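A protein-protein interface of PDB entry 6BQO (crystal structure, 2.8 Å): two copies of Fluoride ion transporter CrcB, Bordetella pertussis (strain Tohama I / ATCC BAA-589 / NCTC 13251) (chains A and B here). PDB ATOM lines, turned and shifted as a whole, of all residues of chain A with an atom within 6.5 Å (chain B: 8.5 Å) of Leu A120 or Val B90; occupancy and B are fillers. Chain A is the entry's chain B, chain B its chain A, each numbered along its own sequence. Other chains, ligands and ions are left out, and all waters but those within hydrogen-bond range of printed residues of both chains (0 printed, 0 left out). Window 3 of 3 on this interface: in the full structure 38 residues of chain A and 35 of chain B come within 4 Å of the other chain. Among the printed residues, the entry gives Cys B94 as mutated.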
ATOM      1  N   TYR A  48      35.451  14.032 -23.961  1.00  0.00           N
ATOM      2  CA  TYR A  48      34.923  12.713 -24.287  1.00  0.00           C
ATOM      3  C   TYR A  48      33.978  12.214 -23.198  1.00  0.00           C
ATOM      4  O   TYR A  48      32.937  11.617 -23.496  1.00  0.00           O
ATOM      5  CB  TYR A  48      36.069  11.724 -24.503  1.00  0.00           C
ATOM      6  CG  TYR A  48      35.603  10.296 -24.659  1.00  0.00           C
ATOM      7  CD1 TYR A  48      35.033   9.857 -25.848  1.00  0.00           C
ATOM      8  CD2 TYR A  48      35.720   9.388 -23.615  1.00  0.00           C
ATOM      9  CE1 TYR A  48      34.598   8.555 -25.993  1.00  0.00           C
ATOM     10  CE2 TYR A  48      35.287   8.082 -23.752  1.00  0.00           C
ATOM     11  CZ  TYR A  48      34.726   7.672 -24.943  1.00  0.00           C
ATOM     12  OH  TYR A  48      34.293   6.372 -25.085  1.00  0.00           O
ATOM     13  N   ILE A  50      32.144  13.936 -20.929  1.00  0.00           N
ATOM     14  CA  ILE A  50      30.863  14.635 -20.871  1.00  0.00           C
ATOM     15  C   ILE A  50      29.933  14.111 -21.957  1.00  0.00           C
ATOM     16  O   ILE A  50      28.721  13.981 -21.747  1.00  0.00           O
ATOM     17  CB  ILE A  50      31.064  16.159 -20.972  1.00  0.00           C
ATOM     18  CG1 ILE A  50      29.768  16.884 -20.599  1.00  0.00           C
ATOM     19  CG2 ILE A  50      31.511  16.554 -22.368  1.00  0.00           C
ATOM     20  CD1 ILE A  50      29.899  18.386 -20.548  1.00  0.00           C
ATOM     21  N   GLY A  51      30.483  13.795 -23.130  1.00  0.00           N
ATOM     22  CA  GLY A  51      29.685  13.131 -24.144  1.00  0.00           C
ATOM     23  C   GLY A  51      29.122  11.815 -23.649  1.00  0.00           C
ATOM     24  O   GLY A  51      27.999  11.437 -23.992  1.00  0.00           O
ATOM     25  N   VAL A  52      29.891  11.104 -22.825  1.00  0.00           N
ATOM     26  CA  VAL A  52      29.411   9.854 -22.248  1.00  0.00           C
ATOM     27  C   VAL A  52      28.357  10.132 -21.185  1.00  0.00           C
ATOM     28  O   VAL A  52      27.275   9.533 -21.187  1.00  0.00           O
ATOM     29  CB  VAL A  52      30.590   9.043 -21.680  1.00  0.00           C
ATOM     30  CG1 VAL A  52      30.090   7.805 -20.958  1.00  0.00           C
ATOM     31  CG2 VAL A  52      31.556   8.666 -22.794  1.00  0.00           C
ATOM     32  N   VAL A  54      26.454  12.801 -20.753  1.00  0.00           N
ATOM     33  CA  VAL A  54      25.226  13.355 -21.318  1.00  0.00           C
ATOM     34  C   VAL A  54      24.383  12.251 -21.947  1.00  0.00           C
ATOM     35  O   VAL A  54      23.152  12.245 -21.829  1.00  0.00           O
ATOM     36  CB  VAL A  54      25.548  14.473 -22.327  1.00  0.00           C
ATOM     37  CG1 VAL A  54      24.332  14.767 -23.189  1.00  0.00           C
ATOM     38  CG2 VAL A  54      25.991  15.734 -21.595  1.00  0.00           C
ATOM     39  N   ALA A  55      25.031  11.293 -22.615  1.00  0.00           N
ATOM     40  CA  ALA A  55      24.290  10.187 -23.214  1.00  0.00           C
ATOM     41  C   ALA A  55      23.679   9.287 -22.147  1.00  0.00           C
ATOM     42  O   ALA A  55      22.541   8.827 -22.292  1.00  0.00           O
ATOM     43  CB  ALA A  55      25.200   9.381 -24.139  1.00  0.00           C
ATOM     44  N   SER A 112      37.976  18.633 -28.740  1.00  0.00           N
ATOM     45  CA  SER A 112      36.938  18.466 -27.727  1.00  0.00           C
ATOM     46  C   SER A 112      35.609  18.085 -28.365  1.00  0.00           C
ATOM     47  O   SER A 112      34.958  17.120 -27.945  1.00  0.00           O
ATOM     48  CB  SER A 112      36.800  19.750 -26.910  1.00  0.00           C
ATOM     49  OG  SER A 112      35.951  19.552 -25.794  1.00  0.00           O
ATOM     50  N   LEU A 113      35.187  18.836 -29.386  1.00  0.00           N
ATOM     51  CA  LEU A 113      33.936  18.531 -30.072  1.00  0.00           C
ATOM     52  C   LEU A 113      33.923  17.092 -30.574  1.00  0.00           C
ATOM     53  O   LEU A 113      32.969  16.344 -30.332  1.00  0.00           O
ATOM     54  CB  LEU A 113      33.729  19.502 -31.234  1.00  0.00           C
ATOM     55  CG  LEU A 113      33.682  20.986 -30.875  1.00  0.00           C
ATOM     56  CD1 LEU A 113      33.581  21.832 -32.135  1.00  0.00           C
ATOM     57  CD2 LEU A 113      32.520  21.268 -29.935  1.00  0.00           C
ATOM     58  N   ALA A 114      34.983  16.690 -31.277  1.00  0.00           N
ATOM     59  CA  ALA A 114      35.069  15.321 -31.774  1.00  0.00           C
ATOM     60  C   ALA A 114      35.009  14.319 -30.629  1.00  0.00           C
ATOM     61  O   ALA A 114      34.289  13.316 -30.703  1.00  0.00           O
ATOM     62  CB  ALA A 114      36.352  15.137 -32.584  1.00  0.00           C
ATOM     63  N   MET A 115      35.764  14.572 -29.557  1.00  0.00           N
ATOM     64  CA  MET A 115      35.745  13.664 -28.414  1.00  0.00           C
ATOM     65  C   MET A 115      34.354  13.577 -27.802  1.00  0.00           C
ATOM     66  O   MET A 115      33.904  12.492 -27.414  1.00  0.00           O
ATOM     67  CB  MET A 115      36.771  14.104 -27.372  1.00  0.00           C
ATOM     68  CG  MET A 115      38.208  13.783 -27.753  1.00  0.00           C
ATOM     69  SD  MET A 115      38.451  12.022 -28.067  1.00  0.00           S
ATOM     70  CE  MET A 115      40.213  11.973 -28.392  1.00  0.00           C
ATOM     71  N   THR A 116      33.655  14.710 -27.702  1.00  0.00           N
ATOM     72  CA  THR A 116      32.278  14.673 -27.224  1.00  0.00           C
ATOM     73  C   THR A 116      31.410  13.821 -28.140  1.00  0.00           C
ATOM     74  O   THR A 116      30.582  13.032 -27.669  1.00  0.00           O
ATOM     75  CB  THR A 116      31.717  16.090 -27.108  1.00  0.00           C
ATOM     76  OG1 THR A 116      32.534  16.855 -26.213  1.00  0.00           O
ATOM     77  CG2 THR A 116      30.293  16.057 -26.577  1.00  0.00           C
ATOM     78  N   GLY A 117      31.593  13.955 -29.453  1.00  0.00           N
ATOM     79  CA  GLY A 117      30.870  13.102 -30.378  1.00  0.00           C
ATOM     80  C   GLY A 117      31.145  11.629 -30.149  1.00  0.00           C
ATOM     81  O   GLY A 117      30.228  10.805 -30.176  1.00  0.00           O
ATOM     82  N   LEU A 118      32.412  11.274 -29.919  1.00  0.00           N
ATOM     83  CA  LEU A 118      32.742   9.879 -29.647  1.00  0.00           C
ATOM     84  C   LEU A 118      32.112   9.410 -28.343  1.00  0.00           C
ATOM     85  O   LEU A 118      31.562   8.304 -28.276  1.00  0.00           O
ATOM     86  CB  LEU A 118      34.257   9.691 -29.609  1.00  0.00           C
ATOM     87  CG  LEU A 118      34.985   9.768 -30.951  1.00  0.00           C
ATOM     88  CD1 LEU A 118      36.475   9.527 -30.761  1.00  0.00           C
ATOM     89  CD2 LEU A 118      34.390   8.771 -31.940  1.00  0.00           C
ATOM     90  N   GLY A 119      32.188  10.230 -27.294  1.00  0.00           N
ATOM     91  CA  GLY A 119      31.510   9.887 -26.054  1.00  0.00           C
ATOM     92  C   GLY A 119      30.037   9.602 -26.265  1.00  0.00           C
ATOM     93  O   GLY A 119      29.505   8.605 -25.770  1.00  0.00           O
ATOM     94  N   LEU A 120      29.356  10.476 -27.010  1.00  0.00           N
ATOM     95  CA  LEU A 120      27.965  10.213 -27.366  1.00  0.00           C
ATOM     96  C   LEU A 120      27.839   8.927 -28.170  1.00  0.00           C
ATOM     97  O   LEU A 120      26.922   8.130 -27.943  1.00  0.00           O
ATOM     98  CB  LEU A 120      27.390  11.391 -28.153  1.00  0.00           C
ATOM     99  CG  LEU A 120      27.202  12.716 -27.413  1.00  0.00           C
ATOM    100  CD1 LEU A 120      26.881  13.821 -28.400  1.00  0.00           C
ATOM    101  CD2 LEU A 120      26.107  12.603 -26.361  1.00  0.00           C
ATOM    102  N   ALA A 121      28.755   8.708 -29.116  1.00  0.00           N
ATOM    103  CA  ALA A 121      28.699   7.504 -29.937  1.00  0.00           C
ATOM    104  C   ALA A 121      29.003   6.255 -29.117  1.00  0.00           C
ATOM    105  O   ALA A 121      28.376   5.209 -29.318  1.00  0.00           O
ATOM    106  CB  ALA A 121      29.669   7.628 -31.113  1.00  0.00           C
ATOM    107  N   THR A 122      29.963   6.344 -28.193  1.00  0.00           N
ATOM    108  CA  THR A 122      30.301   5.195 -27.359  1.00  0.00           C
ATOM    109  C   THR A 122      29.072   4.659 -26.636  1.00  0.00           C
ATOM    110  O   THR A 122      28.780   3.459 -26.686  1.00  0.00           O
ATOM    111  CB  THR A 122      31.383   5.573 -26.346  1.00  0.00           C
ATOM    112  OG1 THR A 122      32.579   5.961 -27.036  1.00  0.00           O
ATOM    113  CG2 THR A 122      31.683   4.394 -25.433  1.00  0.00           C
ATOM    114  N   VAL A 123      28.342   5.540 -25.951  1.00  0.00           N
ATOM    115  CA  VAL A 123      27.147   5.112 -25.229  1.00  0.00           C
ATOM    116  C   VAL A 123      26.086   4.617 -26.203  1.00  0.00           C
ATOM    117  O   VAL A 123      25.555   3.509 -26.059  1.00  0.00           O
ATOM    118  CB  VAL A 123      26.615   6.254 -24.347  1.00  0.00           C
ATOM    119  CG1 VAL A 123      25.354   5.815 -23.619  1.00  0.00           C
ATOM    120  CG2 VAL A 123      27.683   6.701 -23.358  1.00  0.00           C
ATOM    121  N   ARG A 124      25.759   5.432 -27.210  1.00  0.00           N
ATOM    122  CA  ARG A 124      24.785   5.025 -28.217  1.00  0.00           C
ATOM    123  C   ARG A 124      25.130   3.669 -28.819  1.00  0.00           C
ATOM    124  O   ARG A 124      24.242   2.954 -29.299  1.00  0.00           O
ATOM    125  CB  ARG A 124      24.702   6.088 -29.317  1.00  0.00           C
ATOM    126  CG  ARG A 124      23.626   7.150 -29.115  1.00  0.00           C
ATOM    127  CD  ARG A 124      23.502   7.588 -27.662  1.00  0.00           C
ATOM    128  NE  ARG A 124      22.712   8.812 -27.530  1.00  0.00           N
ATOM    129  CZ  ARG A 124      21.935   9.096 -26.488  1.00  0.00           C
ATOM    130  NH1 ARG A 124      21.823   8.237 -25.484  1.00  0.00           N
ATOM    131  NH2 ARG A 124      21.257  10.236 -26.457  1.00  0.00           N
ATOM    132  N   LEU A 125      26.410   3.296 -28.794  1.00  0.00           N
ATOM    133  CA  LEU A 125      26.854   2.051 -29.407  1.00  0.00           C
ATOM    134  C   LEU A 125      26.481   0.837 -28.562  1.00  0.00           C
ATOM    135  O   LEU A 125      26.058  -0.192 -29.101  1.00  0.00           O
ATOM    136  CB  LEU A 125      28.368   2.098 -29.624  1.00  0.00           C
ATOM    137  CG  LEU A 125      28.983   1.063 -30.563  1.00  0.00           C
ATOM    138  CD1 LEU A 125      28.530   1.325 -31.990  1.00  0.00           C
ATOM    139  CD2 LEU A 125      30.504   1.077 -30.459  1.00  0.00           C
ATOM    140  N   PHE B  82      35.680  23.535 -20.471  1.00  0.00           N
ATOM    141  CA  PHE B  82      35.668  23.142 -21.874  1.00  0.00           C
ATOM    142  C   PHE B  82      34.651  22.045 -22.153  1.00  0.00           C
ATOM    143  O   PHE B  82      34.034  22.032 -23.223  1.00  0.00           O
ATOM    144  CB  PHE B  82      37.061  22.671 -22.307  1.00  0.00           C
ATOM    145  CG  PHE B  82      37.530  23.276 -23.599  1.00  0.00           C
ATOM    146  CD1 PHE B  82      37.039  22.823 -24.812  1.00  0.00           C
ATOM    147  CD2 PHE B  82      38.461  24.301 -23.601  1.00  0.00           C
ATOM    148  CE1 PHE B  82      37.468  23.382 -26.003  1.00  0.00           C
ATOM    149  CE2 PHE B  82      38.895  24.863 -24.786  1.00  0.00           C
ATOM    150  CZ  PHE B  82      38.397  24.404 -25.988  1.00  0.00           C
ATOM    151  N   SER B  83      34.450  21.135 -21.196  1.00  0.00           N
ATOM    152  CA  SER B  83      33.506  20.039 -21.388  1.00  0.00           C
ATOM    153  C   SER B  83      32.090  20.560 -21.611  1.00  0.00           C
ATOM    154  O   SER B  83      31.387  20.112 -22.524  1.00  0.00           O
ATOM    155  CB  SER B  83      33.553  19.099 -20.184  1.00  0.00           C
ATOM    156  OG  SER B  83      33.269  19.798 -18.984  1.00  0.00           O
ATOM    157  N   THR B  84      31.648  21.504 -20.775  1.00  0.00           N
ATOM    158  CA  THR B  84      30.304  22.053 -20.931  1.00  0.00           C
ATOM    159  C   THR B  84      30.176  22.857 -22.218  1.00  0.00           C
ATOM    160  O   THR B  84      29.074  22.982 -22.766  1.00  0.00           O
ATOM    161  CB  THR B  84      29.942  22.924 -19.726  1.00  0.00           C
ATOM    162  OG1 THR B  84      30.006  22.140 -18.529  1.00  0.00           O
ATOM    163  CG2 THR B  84      28.540  23.490 -19.879  1.00  0.00           C
ATOM    164  N   PHE B  85      31.286  23.405 -22.713  1.00  0.00           N
ATOM    165  CA  PHE B  85      31.250  24.183 -23.947  1.00  0.00           C
ATOM    166  C   PHE B  85      31.045  23.283 -25.161  1.00  0.00           C
ATOM    167  O   PHE B  85      30.215  23.574 -26.031  1.00  0.00           O
ATOM    168  CB  PHE B  85      32.537  24.995 -24.085  1.00  0.00           C
ATOM    169  CG  PHE B  85      32.833  25.434 -25.490  1.00  0.00           C
ATOM    170  CD1 PHE B  85      32.191  26.531 -26.038  1.00  0.00           C
ATOM    171  CD2 PHE B  85      33.763  24.754 -26.259  1.00  0.00           C
ATOM    172  CE1 PHE B  85      32.467  26.936 -27.332  1.00  0.00           C
ATOM    173  CE2 PHE B  85      34.044  25.155 -27.554  1.00  0.00           C
ATOM    174  CZ  PHE B  85      33.396  26.246 -28.090  1.00  0.00           C
ATOM    175  N   SER B  86      31.801  22.187 -25.245  1.00  0.00           N
ATOM    176  CA  SER B  86      31.686  21.320 -26.412  1.00  0.00           C
ATOM    177  C   SER B  86      30.392  20.520 -26.383  1.00  0.00           C
ATOM    178  O   SER B  86      29.810  20.248 -27.439  1.00  0.00           O
ATOM    179  CB  SER B  86      32.898  20.391 -26.514  1.00  0.00           C
ATOM    180  OG  SER B  86      33.030  19.568 -25.371  1.00  0.00           O
ATOM    181  N   ALA B  87      29.922  20.143 -25.193  1.00  0.00           N
ATOM    182  CA  ALA B  87      28.605  19.523 -25.086  1.00  0.00           C
ATOM    183  C   ALA B  87      27.534  20.433 -25.670  1.00  0.00           C
ATOM    184  O   ALA B  87      26.729  20.011 -26.507  1.00  0.00           O
ATOM    185  CB  ALA B  87      28.294  19.193 -23.628  1.00  0.00           C
ATOM    186  N   GLU B  88      27.516  21.696 -25.243  1.00  0.00           N
ATOM    187  CA  GLU B  88      26.547  22.644 -25.781  1.00  0.00           C
ATOM    188  C   GLU B  88      26.724  22.808 -27.284  1.00  0.00           C
ATOM    189  O   GLU B  88      25.755  22.739 -28.047  1.00  0.00           O
ATOM    190  CB  GLU B  88      26.682  23.986 -25.063  1.00  0.00           C
ATOM    191  CG  GLU B  88      26.352  23.921 -23.580  1.00  0.00           C
ATOM    192  CD  GLU B  88      26.875  25.120 -22.813  1.00  0.00           C
ATOM    193  OE1 GLU B  88      27.679  25.888 -23.384  1.00  0.00           O
ATOM    194  OE2 GLU B  88      26.482  25.292 -21.638  1.00  0.00           O
ATOM    195  N   THR B  89      27.964  23.018 -27.729  1.00  0.00           N
ATOM    196  CA  THR B  89      28.220  23.205 -29.155  1.00  0.00           C
ATOM    197  C   THR B  89      27.842  21.959 -29.949  1.00  0.00           C
ATOM    198  O   THR B  89      27.191  22.049 -30.995  1.00  0.00           O
ATOM    199  CB  THR B  89      29.690  23.566 -29.380  1.00  0.00           C
ATOM    200  OG1 THR B  89      30.038  24.686 -28.556  1.00  0.00           O
ATOM    201  CG2 THR B  89      29.932  23.928 -30.834  1.00  0.00           C
ATOM    202  N   VAL B  90      28.243  20.781 -29.463  1.00  0.00           N
ATOM    203  CA  VAL B  90      27.887  19.540 -30.148  1.00  0.00           C
ATOM    204  C   VAL B  90      26.377  19.364 -30.194  1.00  0.00           C
ATOM    205  O   VAL B  90      25.836  18.809 -31.158  1.00  0.00           O
ATOM    206  CB  VAL B  90      28.568  18.335 -29.471  1.00  0.00           C
ATOM    207  CG1 VAL B  90      27.957  17.036 -29.970  1.00  0.00           C
ATOM    208  CG2 VAL B  90      30.067  18.352 -29.731  1.00  0.00           C
ATOM    209  N   ASP B  91      25.670  19.822 -29.158  1.00  0.00           N
ATOM    210  CA  ASP B  91      24.216  19.724 -29.170  1.00  0.00           C
ATOM    211  C   ASP B  91      23.614  20.624 -30.240  1.00  0.00           C
ATOM    212  O   ASP B  91      22.648  20.244 -30.911  1.00  0.00           O
ATOM    213  CB  ASP B  91      23.656  20.070 -27.790  1.00  0.00           C
ATOM    214  CG  ASP B  91      22.163  19.817 -27.685  1.00  0.00           C
ATOM    215  OD1 ASP B  91      21.720  18.708 -28.052  1.00  0.00           O
ATOM    216  OD2 ASP B  91      21.433  20.723 -27.229  1.00  0.00           O
ATOM    217  N   MET B  92      24.177  21.821 -30.421  1.00  0.00           N
ATOM    218  CA  MET B  92      23.717  22.703 -31.488  1.00  0.00           C
ATOM    219  C   MET B  92      23.883  22.040 -32.850  1.00  0.00           C
ATOM    220  O   MET B  92      22.970  22.070 -33.684  1.00  0.00           O
ATOM    221  CB  MET B  92      24.477  24.029 -31.430  1.00  0.00           C
ATOM    222  CG  MET B  92      24.121  24.903 -30.237  1.00  0.00           C
ATOM    223  SD  MET B  92      25.363  26.174 -29.918  1.00  0.00           S
ATOM    224  CE  MET B  92      24.531  27.187 -28.699  1.00  0.00           C
ATOM    225  N   LEU B  93      25.049  21.438 -33.098  1.00  0.00           N
ATOM    226  CA  LEU B  93      25.244  20.710 -34.347  1.00  0.00           C
ATOM    227  C   LEU B  93      24.266  19.548 -34.457  1.00  0.00           C
ATOM    228  O   LEU B  93      23.731  19.273 -35.538  1.00  0.00           O
ATOM    229  CB  LEU B  93      26.683  20.202 -34.449  1.00  0.00           C
ATOM    230  CG  LEU B  93      27.824  21.217 -34.344  1.00  0.00           C
ATOM    231  CD1 LEU B  93      29.161  20.497 -34.363  1.00  0.00           C
ATOM    232  CD2 LEU B  93      27.758  22.243 -35.460  1.00  0.00           C
ATOM    233  N   CYS B  94      24.020  18.856 -33.343  1.00  0.00           N
ATOM    234  CA  CYS B  94      23.079  17.740 -33.343  1.00  0.00           C
ATOM    235  C   CYS B  94      21.715  18.169 -33.869  1.00  0.00           C
ATOM    236  O   CYS B  94      21.108  17.477 -34.695  1.00  0.00           O
ATOM    237  CB  CYS B  94      22.962  17.163 -31.931  1.00  0.00           C
ATOM    238  SG  CYS B  94      21.587  16.015 -31.681  1.00  0.00           S
ATOM    239  N   ARG B  95      21.215  19.312 -33.401  1.00  0.00           N
ATOM    240  CA  ARG B  95      19.903  19.784 -33.823  1.00  0.00           C
ATOM    241  C   ARG B  95      19.933  20.511 -35.161  1.00  0.00           C
ATOM    242  O   ARG B  95      18.867  20.851 -35.684  1.00  0.00           O
ATOM    243  CB  ARG B  95      19.303  20.698 -32.751  1.00  0.00           C
ATOM    244  CG  ARG B  95      19.239  20.064 -31.369  1.00  0.00           C
ATOM    245  CD  ARG B  95      18.459  20.936 -30.398  1.00  0.00           C
ATOM    246  NE  ARG B  95      18.898  22.327 -30.440  1.00  0.00           N
ATOM    247  CZ  ARG B  95      19.850  22.832 -29.665  1.00  0.00           C
ATOM    248  NH1 ARG B  95      20.468  22.058 -28.783  1.00  0.00           N
ATOM    249  NH2 ARG B  95      20.186  24.111 -29.770  1.00  0.00           N
ATOM    250  N   GLY B  96      21.116  20.761 -35.721  1.00  0.00           N
ATOM    251  CA  GLY B  96      21.237  21.332 -37.044  1.00  0.00           C
ATOM    252  C   GLY B  96      21.531  22.815 -37.103  1.00  0.00           C
ATOM    253  O   GLY B  96      21.750  23.339 -38.201  1.00  0.00           O
ATOM    254  N   VAL B  97      21.543  23.511 -35.969  1.00  0.00           N
ATOM    255  CA  VAL B  97      21.818  24.945 -35.962  1.00  0.00           C
ATOM    256  C   VAL B  97      23.315  25.180 -36.124  1.00  0.00           C
ATOM    257  O   VAL B  97      24.003  25.557 -35.168  1.00  0.00           O
ATOM    258  CB  VAL B  97      21.288  25.608 -34.678  1.00  0.00           C
ATOM    259  CG1 VAL B  97      19.781  25.768 -34.749  1.00  0.00           C
ATOM    260  CG2 VAL B  97      21.677  24.787 -33.460  1.00  0.00           C
ATOM    261  N   TYR B  98      23.830  24.970 -37.339  1.00  0.00           N
ATOM    262  CA  TYR B  98      25.261  25.139 -37.572  1.00  0.00           C
ATOM    263  C   TYR B  98      25.691  26.593 -37.435  1.00  0.00           C
ATOM    264  O   TYR B  98      26.814  26.866 -36.992  1.00  0.00           O
ATOM    265  CB  TYR B  98      25.641  24.610 -38.955  1.00  0.00           C
ATOM    266  CG  TYR B  98      25.610  23.104 -39.074  1.00  0.00           C
ATOM    267  CD1 TYR B  98      25.286  22.308 -37.985  1.00  0.00           C
ATOM    268  CD2 TYR B  98      25.918  22.479 -40.274  1.00  0.00           C
ATOM    269  CE1 TYR B  98      25.261  20.932 -38.090  1.00  0.00           C
ATOM    270  CE2 TYR B  98      25.898  21.105 -40.388  1.00  0.00           C
ATOM    271  CZ  TYR B  98      25.569  20.337 -39.295  1.00  0.00           C
ATOM    272  OH  TYR B  98      25.546  18.966 -39.406  1.00  0.00           O
ATOM    273  N   ALA B 101      26.183  27.194 -33.637  1.00  0.00           N
ATOM    274  CA  ALA B 101      27.393  26.522 -33.176  1.00  0.00           C
ATOM    275  C   ALA B 101      28.640  27.274 -33.626  1.00  0.00           C
ATOM    276  O   ALA B 101      29.548  27.533 -32.827  1.00  0.00           O
ATOM    277  CB  ALA B 101      27.415  25.079 -33.683  1.00  0.00           C
ATOM    278  N   TYR B 104      28.857  30.382 -31.769  1.00  0.00           N
ATOM    279  CA  TYR B 104      29.167  30.118 -30.368  1.00  0.00           C
ATOM    280  C   TYR B 104      30.629  29.732 -30.189  1.00  0.00           C
ATOM    281  O   TYR B 104      31.288  30.198 -29.252  1.00  0.00           O
ATOM    282  CB  TYR B 104      28.252  29.023 -29.822  1.00  0.00           C
ATOM    283  CG  TYR B 104      28.459  28.731 -28.351  1.00  0.00           C
ATOM    284  CD1 TYR B 104      28.359  29.740 -27.404  1.00  0.00           C
ATOM    285  CD2 TYR B 104      28.738  27.444 -27.910  1.00  0.00           C
ATOM    286  CE1 TYR B 104      28.541  29.481 -26.059  1.00  0.00           C
ATOM    287  CE2 TYR B 104      28.920  27.174 -26.565  1.00  0.00           C
ATOM    288  CZ  TYR B 104      28.820  28.198 -25.644  1.00  0.00           C
ATOM    289  OH  TYR B 104      28.999  27.938 -24.305  1.00  0.00           O
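The side-chain hydroxyl (OG) of Ser A112 lies within hydrogen-bond range of the side-chain hydroxyl (OG) of Ser B86 (3.0 Å). OG of Ser B86 is in hydrogen-bond range of OG1 of Thr A116 (2.9 Å).
The backbone carbonyl oxygen (O) of Phe B82 sits at hydrogen-bond distance from the side-chain hydroxyl (OG) of Ser B86, 3.4 Å away. The side-chain hydroxyl of Ser B86 is in hydrogen-bond range of the backbone carbonyl oxygen of Ser B83. The backbone carbonyl oxygen of Phe B85 is in hydrogen-bond range of the side-chain hydroxyl of Thr B89, at 2.8 Å. The backbone carbonyl oxygen (O) of Gly A51 lies close to the backbone NH (N) of Leu A120 (3.4 Å). The side-chain hydroxyl of Thr A116 is in hydrogen-bond range of the backbone carbonyl oxygen of Ser A112 (3.0 Å).
Ser B83 touches Ile A50. Ile A50 touches Thr B84. Ala B87 touches Ile A50. OG of Ser A112 touches CD1 of Phe B82, 3.6 Å away. Leu A113 touches Ser B86 (CD2 to CB, 3.6 Å). Leu A113 touches Thr B89. O of Leu A113 touches CG2 of Val B90, 3.6 Å away. Thr A116 touches Val B90. CG1 of Val B90 touches CD1 of Leu A120, 3.7 Å away.
Leu A120 touches just one residue of chain B: Val B90. Of chain A, only Leu A113 (3.6 Å), Thr A116 (3.8 Å) and Leu A120 (3.7 Å) come within 4 Å of Val B90. Gly A119 touches none of the printed residues of chain B. Printed residues of chain B within 4 Å of Ser A112: Phe B82 and Ser B86. Of the printed residues of chain B, Ile A50 touches Ser B83 (3.0 Å), Thr B84 (3.6 Å) and Ala B87 (3.6 Å). Gly A51 touches none of the printed residues of chain B. Thr A122 touches none of the printed residues of chain B. The nearest printed residue of chain B that does not touch Ile A50 is Ser B86 (4.5 Å).
Of the 19 printed residues of chain B, 7 touch a printed residue of chain A. Hydrophobic or aromatic side chains of chain B that line the printed part of chain A: Phe B82, Ala B87 and Val B90. Of the 20 printed residues of chain A, 5 touch a printed residue of chain B. Printed residues of chain A that touch a printed residue of chain B: Ile A50, Ser A112, Leu A113, Thr A116 and Leu A120. Hydrophobic or aromatic side chains of chain A that line the printed part of chain B: Ile A50, Leu A113 and Leu A120. Among the printed residues, no Asp or Glu carboxylate lies within 4 Å of a Lys or Arg side-chain nitrogen of the other chain.
No position is printed for both chains.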
